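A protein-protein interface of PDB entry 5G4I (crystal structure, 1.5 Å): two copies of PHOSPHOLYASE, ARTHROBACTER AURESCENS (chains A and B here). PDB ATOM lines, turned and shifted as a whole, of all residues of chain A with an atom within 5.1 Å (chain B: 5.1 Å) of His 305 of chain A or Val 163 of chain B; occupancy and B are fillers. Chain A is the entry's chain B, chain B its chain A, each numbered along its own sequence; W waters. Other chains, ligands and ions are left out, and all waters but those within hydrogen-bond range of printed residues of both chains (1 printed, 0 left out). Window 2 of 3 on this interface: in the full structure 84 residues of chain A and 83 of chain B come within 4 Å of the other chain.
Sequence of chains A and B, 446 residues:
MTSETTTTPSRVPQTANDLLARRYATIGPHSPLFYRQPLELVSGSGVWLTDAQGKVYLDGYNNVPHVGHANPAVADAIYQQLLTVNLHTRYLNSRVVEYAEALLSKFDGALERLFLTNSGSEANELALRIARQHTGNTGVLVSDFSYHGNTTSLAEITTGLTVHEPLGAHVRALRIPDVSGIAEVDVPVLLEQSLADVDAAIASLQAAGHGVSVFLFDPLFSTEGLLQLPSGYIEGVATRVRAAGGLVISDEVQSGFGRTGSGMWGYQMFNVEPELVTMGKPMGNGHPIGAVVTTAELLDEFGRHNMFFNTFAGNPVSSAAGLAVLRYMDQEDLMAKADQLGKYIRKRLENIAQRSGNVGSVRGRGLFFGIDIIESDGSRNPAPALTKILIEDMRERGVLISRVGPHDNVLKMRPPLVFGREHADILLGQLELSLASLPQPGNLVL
The side-chain amide oxygen (OD1) of Asn 306 of chain A is in hydrogen-bond range of the guanidinium group (NH2) of Arg 129 of chain A (3.2 Å). ND2 of Asn 306 of chain A lies within hydrogen-bond range of OE1 of Gln 133 of chain A, 2.9 Å away. The backbone carbonyl oxygen (O) of Glu 301 of chain A sits close to a ring nitrogen (ND1) of His 305 of chain A (3.5 Å). The backbone carbonyl oxygen (O) of Phe 302 of chain A lies within hydrogen-bond range of the side-chain amide nitrogen (ND2) of Asn 306 of chain A.
Water W1 bridges the backbone carbonyl oxygen (O) of Gln 133 of chain A (2.7 Å) and a ring nitrogen (NE2) of His 164 of chain B (3.4 Å).
Of the 7 printed residues of chain B, 6 touch a printed residue of chain A. Printed residues of chain B that touch a printed residue of chain A: Ala 155, Leu 161, Thr 162, Val 163, His 164 and Glu 165. Of the 9 printed residues of chain A, 5 touch a printed residue of chain B. Printed residues of chain A that touch a printed residue of chain B: Arg 129, Gln 133, His 305, Asn 306 and Met 307. Hydrophobic or aromatic side chains of chain A that line the printed part of chain B: His 305 and Met 307. Among the printed residues, Asp or Glu carboxylates within 4 Å of a Lys or Arg side-chain nitrogen of the other chain: Arg 129 of chain A with Glu 165 of chain B.
O of Thr 162 of chain B is in hydrogen-bond range of N of Met 307 of chain A. O of His 305 of chain A sits at hydrogen-bond distance from N of His 164 of chain B, 3.3 Å away. The backbone NH (N) of His 164 of chain B lies within hydrogen-bond range of the side-chain amide oxygen (OD1) of Asn 306 of chain A (2.9 Å). The side-chain carboxylate of Glu 165 of chain B is in salt-bridge range of the guanidinium group of Arg 129 of chain A (2.9 Å). The side-chain amide nitrogen (NE2) of Gln 133 of chain A sits at hydrogen-bond distance from the side-chain carboxylate (OE2) of Glu 165 of chain B (2.9 Å).
Glu 301 of chain A touches none of the printed residues of chain B. Of chain B, only Val 163 (3.7 Å) and His 164 (3.3 Å) come within 4 Å of His 305 of chain A. Of the printed residues of chain A, Ala 155 of chain B touches Arg 129. Val 163 of chain B touches three residues of chain A. Of the printed residues of chain A, His 164 of chain B touches Gln 133, His 305 and Asn 306. Of the printed residues of chain A, Glu 165 of chain B touches Arg 129 (2.9 Å), Gln 133 (2.9 Å) and Asn 306 (3.6 Å). The nearest residue of chain A that does not touch Val 163 of chain B is Met 307 of chain A (5.0 Å).
Among the printed residues, pairs that only touch across the chains: Arg 129 of chain A with Ala 155 of chain B, Arg 129 of chain A with Val 163 of chain B, Gln 133 of chain A with His 164 of chain B, His 305 of chain A with Val 163 of chain B, Asn 306 of chain A with Thr 162 of chain B, Asn 306 of chain A with Val 163 of chain B, Asn 306 of chain A with Glu 165 of chain B and Met 307 of chain A with Leu 161 of chain B.
No position is printed for both chains.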
ATOM      1  N   ARG A 129     -12.160   4.514 -25.898  1.00  0.00           N
ATOM      2  CA  ARG A 129     -11.333   5.753 -26.019  1.00  0.00           C
ATOM      3  C   ARG A 129     -11.400   6.333 -27.479  1.00  0.00           C
ATOM      4  O   ARG A 129     -11.640   7.529 -27.678  1.00  0.00           O
ATOM      5  CB  ARG A 129      -9.902   5.498 -25.508  1.00  0.00           C
ATOM      6  CG  ARG A 129      -9.020   6.735 -25.477  1.00  0.00           C
ATOM      7  CD  ARG A 129      -7.581   6.462 -24.901  1.00  0.00           C
ATOM      8  NE  ARG A 129      -6.744   7.661 -25.007  1.00  0.00           N
ATOM      9  CZ  ARG A 129      -5.440   7.690 -25.232  1.00  0.00           C
ATOM     10  NH1 ARG A 129      -4.715   6.578 -25.140  1.00  0.00           N
ATOM     11  NH2 ARG A 129      -4.802   8.829 -25.412  1.00  0.00           N
ATOM     12  N   GLN A 133     -13.385   9.988 -28.456  1.00  0.00           N
ATOM     13  CA  GLN A 133     -12.691  11.063 -29.190  1.00  0.00           C
ATOM     14  C   GLN A 133     -13.360  11.321 -30.549  1.00  0.00           C
ATOM     15  O   GLN A 133     -13.463  12.494 -30.986  1.00  0.00           O
ATOM     16  CB  GLN A 133     -11.193  10.746 -29.439  1.00  0.00           C
ATOM     17  CG  GLN A 133     -10.354  10.614 -28.140  1.00  0.00           C
ATOM     18  CD  GLN A 133      -8.859  10.565 -28.402  1.00  0.00           C
ATOM     19  OE1 GLN A 133      -8.381  10.736 -29.547  1.00  0.00           O
ATOM     20  NE2 GLN A 133      -8.054  10.274 -27.318  1.00  0.00           N
ATOM     21  N   GLU A 301      -7.486   8.622 -37.964  1.00  0.00           N
ATOM     22  CA  GLU A 301      -7.873   9.758 -37.137  1.00  0.00           C
ATOM     23  C   GLU A 301      -7.213   9.659 -35.715  1.00  0.00           C
ATOM     24  O   GLU A 301      -6.668  10.633 -35.201  1.00  0.00           O
ATOM     25  CB  GLU A 301      -9.379   9.897 -37.029  1.00  0.00           C
ATOM     26  CG  GLU A 301      -9.872  10.958 -36.127  1.00  0.00           C
ATOM     27  CD  GLU A 301     -11.370  10.941 -35.940  1.00  0.00           C
ATOM     28  OE1 GLU A 301     -12.026   9.920 -35.956  1.00  0.00           O
ATOM     29  OE2 GLU A 301     -11.940  12.036 -35.788  1.00  0.00           O
ATOM     30  N   PHE A 302      -7.358   8.482 -35.099  1.00  0.00           N
ATOM     31  CA  PHE A 302      -6.855   8.336 -33.715  1.00  0.00           C
ATOM     32  C   PHE A 302      -5.325   8.475 -33.730  1.00  0.00           C
ATOM     33  O   PHE A 302      -4.791   9.127 -32.788  1.00  0.00           O
ATOM     34  CB  PHE A 302      -7.244   6.958 -33.186  1.00  0.00           C
ATOM     35  CG  PHE A 302      -6.973   6.749 -31.703  1.00  0.00           C
ATOM     36  CD1 PHE A 302      -7.727   7.363 -30.716  1.00  0.00           C
ATOM     37  CD2 PHE A 302      -5.859   5.941 -31.310  1.00  0.00           C
ATOM     38  CE1 PHE A 302      -7.422   7.180 -29.353  1.00  0.00           C
ATOM     39  CE2 PHE A 302      -5.591   5.776 -29.960  1.00  0.00           C
ATOM     40  CZ  PHE A 302      -6.390   6.360 -29.002  1.00  0.00           C
ATOM     41  N   GLY A 303      -4.575   7.945 -34.759  1.00  0.00           N
ATOM     42  CA  GLY A 303      -3.094   8.107 -34.798  1.00  0.00           C
ATOM     43  C   GLY A 303      -2.648   9.512 -35.079  1.00  0.00           C
ATOM     44  O   GLY A 303      -1.578   9.936 -34.619  1.00  0.00           O
ATOM     45  N   ARG A 304      -3.473  10.317 -35.803  1.00  0.00           N
ATOM     46  CA  ARG A 304      -3.104  11.735 -36.031  1.00  0.00           C
ATOM     47  C   ARG A 304      -3.206  12.506 -34.770  1.00  0.00           C
ATOM     48  O   ARG A 304      -2.536  13.502 -34.599  1.00  0.00           O
ATOM     49  CB  ARG A 304      -4.006  12.374 -37.082  1.00  0.00           C
ATOM     50  CG  ARG A 304      -3.693  11.935 -38.511  1.00  0.00           C
ATOM     51  CD  ARG A 304      -4.491  12.822 -39.582  1.00  0.00           C
ATOM     52  NE  ARG A 304      -5.888  13.173 -39.264  1.00  0.00           N
ATOM     53  CZ  ARG A 304      -6.948  12.433 -39.607  1.00  0.00           C
ATOM     54  NH1 ARG A 304      -6.816  11.345 -40.307  1.00  0.00           N
ATOM     55  NH2 ARG A 304      -8.187  12.792 -39.257  1.00  0.00           N
ATOM     56  N   HIS A 305      -4.086  12.066 -33.855  1.00  0.00           N
ATOM     57  CA  HIS A 305      -4.453  12.808 -32.647  1.00  0.00           C
ATOM     58  C   HIS A 305      -3.744  12.346 -31.369  1.00  0.00           C
ATOM     59  O   HIS A 305      -3.820  13.076 -30.325  1.00  0.00           O
ATOM     60  CB  HIS A 305      -5.965  12.720 -32.403  1.00  0.00           C
ATOM     61  CG  HIS A 305      -6.817  13.445 -33.405  1.00  0.00           C
ATOM     62  ND1 HIS A 305      -8.186  13.202 -33.469  1.00  0.00           N
ATOM     63  CD2 HIS A 305      -6.543  14.445 -34.252  1.00  0.00           C
ATOM     64  CE1 HIS A 305      -8.705  14.047 -34.370  1.00  0.00           C
ATOM     65  NE2 HIS A 305      -7.726  14.744 -34.904  1.00  0.00           N
ATOM     66  N   ASN A 306      -3.059  11.191 -31.429  1.00  0.00           N
ATOM     67  CA  ASN A 306      -2.450  10.651 -30.194  1.00  0.00           C
ATOM     68  C   ASN A 306      -1.148   9.904 -30.554  1.00  0.00           C
ATOM     69  O   ASN A 306      -1.130   9.125 -31.536  1.00  0.00           O
ATOM     70  CB  ASN A 306      -3.348   9.627 -29.490  1.00  0.00           C
ATOM     71  CG  ASN A 306      -4.759  10.135 -29.154  1.00  0.00           C
ATOM     72  OD1 ASN A 306      -5.007  10.684 -28.016  1.00  0.00           O
ATOM     73  ND2 ASN A 306      -5.669  10.041 -30.096  1.00  0.00           N
ATOM     74  N   MET A 307      -0.101  10.082 -29.752  1.00  0.00           N
ATOM     75  CA  MET A 307       1.144   9.246 -29.907  1.00  0.00           C
ATOM     76  C   MET A 307       0.861   7.913 -29.120  1.00  0.00           C
ATOM     77  O   MET A 307       1.415   7.649 -27.996  1.00  0.00           O
ATOM     78  CB  MET A 307       2.394   9.988 -29.403  1.00  0.00           C
ATOM     79  CG  MET A 307       3.689   9.192 -29.475  1.00  0.00           C
ATOM     80  SD  MET A 307       3.917   7.898 -30.824  1.00  0.00           S
ATOM     81  CE  MET A 307       4.273   8.896 -32.258  1.00  0.00           C
ATOM     82  N   ALA B 155      -4.125   8.663 -19.942  1.00  0.00           N
ATOM     83  CA  ALA B 155      -4.080   9.766 -20.871  1.00  0.00           C
ATOM     84  C   ALA B 155      -4.435  11.100 -20.250  1.00  0.00           C
ATOM     85  O   ALA B 155      -3.757  12.087 -20.547  1.00  0.00           O
ATOM     86  CB  ALA B 155      -5.047   9.480 -22.038  1.00  0.00           C
ATOM     87  N   THR B 158      -1.285  12.532 -18.607  1.00  0.00           N
ATOM     88  CA  THR B 158      -0.060  12.521 -19.401  1.00  0.00           C
ATOM     89  C   THR B 158       0.446  13.931 -19.773  1.00  0.00           C
ATOM     90  O   THR B 158      -0.313  14.725 -20.346  1.00  0.00           O
ATOM     91  CB  THR B 158      -0.257  11.687 -20.682  1.00  0.00           C
ATOM     92  OG1 THR B 158      -0.532  10.302 -20.328  1.00  0.00           O
ATOM     93  CG2 THR B 158       0.931  11.704 -21.574  1.00  0.00           C
ATOM     94  N   LEU B 161       4.005  13.333 -23.514  1.00  0.00           N
ATOM     95  CA  LEU B 161       3.714  12.807 -24.830  1.00  0.00           C
ATOM     96  C   LEU B 161       2.378  13.420 -25.324  1.00  0.00           C
ATOM     97  O   LEU B 161       1.529  13.813 -24.482  1.00  0.00           O
ATOM     98  CB  LEU B 161       3.684  11.242 -24.573  1.00  0.00           C
ATOM     99  CG  LEU B 161       3.187  10.237 -25.466  1.00  0.00           C
ATOM    100  CD1 LEU B 161       3.922   8.916 -25.397  1.00  0.00           C
ATOM    101  CD2 LEU B 161       1.695  10.080 -25.243  1.00  0.00           C
ATOM    102  N   THR B 162       2.167  13.528 -26.670  1.00  0.00           N
ATOM    103  CA  THR B 162       0.950  14.140 -27.180  1.00  0.00           C
ATOM    104  C   THR B 162      -0.277  13.160 -27.099  1.00  0.00           C
ATOM    105  O   THR B 162      -0.226  12.029 -27.630  1.00  0.00           O
ATOM    106  CB  THR B 162       1.157  14.544 -28.670  1.00  0.00           C
ATOM    107  OG1 THR B 162       2.138  15.541 -28.687  1.00  0.00           O
ATOM    108  CG2 THR B 162      -0.157  15.140 -29.260  1.00  0.00           C
ATOM    109  N   VAL B 163      -1.347  13.629 -26.447  1.00  0.00           N
ATOM    110  CA  VAL B 163      -2.646  12.952 -26.425  1.00  0.00           C
ATOM    111  C   VAL B 163      -3.795  13.953 -26.724  1.00  0.00           C
ATOM    112  O   VAL B 163      -3.599  15.178 -26.521  1.00  0.00           O
ATOM    113  CB  VAL B 163      -2.913  12.221 -25.073  1.00  0.00           C
ATOM    114  CG1 VAL B 163      -1.927  11.100 -24.844  1.00  0.00           C
ATOM    115  CG2 VAL B 163      -2.977  13.180 -23.888  1.00  0.00           C
ATOM    116  N   HIS B 164      -4.900  13.446 -27.246  1.00  0.00           N
ATOM    117  CA  HIS B 164      -6.067  14.347 -27.551  1.00  0.00           C
ATOM    118  C   HIS B 164      -6.710  14.843 -26.297  1.00  0.00           C
ATOM    119  O   HIS B 164      -7.266  15.974 -26.260  1.00  0.00           O
ATOM    120  CB  HIS B 164      -7.050  13.507 -28.394  1.00  0.00           C
ATOM    121  CG  HIS B 164      -8.242  14.253 -28.912  1.00  0.00           C
ATOM    122  ND1 HIS B 164      -8.251  14.969 -30.092  1.00  0.00           N
ATOM    123  CD2 HIS B 164      -9.491  14.292 -28.428  1.00  0.00           C
ATOM    124  CE1 HIS B 164      -9.474  15.431 -30.303  1.00  0.00           C
ATOM    125  NE2 HIS B 164     -10.238  15.055 -29.290  1.00  0.00           N
ATOM    126  N   GLU B 165      -6.746  14.038 -25.223  1.00  0.00           N
ATOM    127  CA  GLU B 165      -7.420  14.448 -23.973  1.00  0.00           C
ATOM    128  C   GLU B 165      -6.761  15.685 -23.365  1.00  0.00           C
ATOM    129  O   GLU B 165      -5.530  15.691 -23.185  1.00  0.00           O
ATOM    130  CB  GLU B 165      -7.313  13.333 -22.898  1.00  0.00           C
ATOM    131  CG  GLU B 165      -8.134  12.071 -23.245  1.00  0.00           C
ATOM    132  CD  GLU B 165      -7.567  11.046 -24.231  1.00  0.00           C
ATOM    133  OE1 GLU B 165      -6.459  11.250 -24.781  1.00  0.00           O
ATOM    134  OE2 GLU B 165      -8.309  10.029 -24.479  1.00  0.00           O
HETATM  135  O   HOH W   1     -13.597  14.832 -29.606  1.00  0.00           O
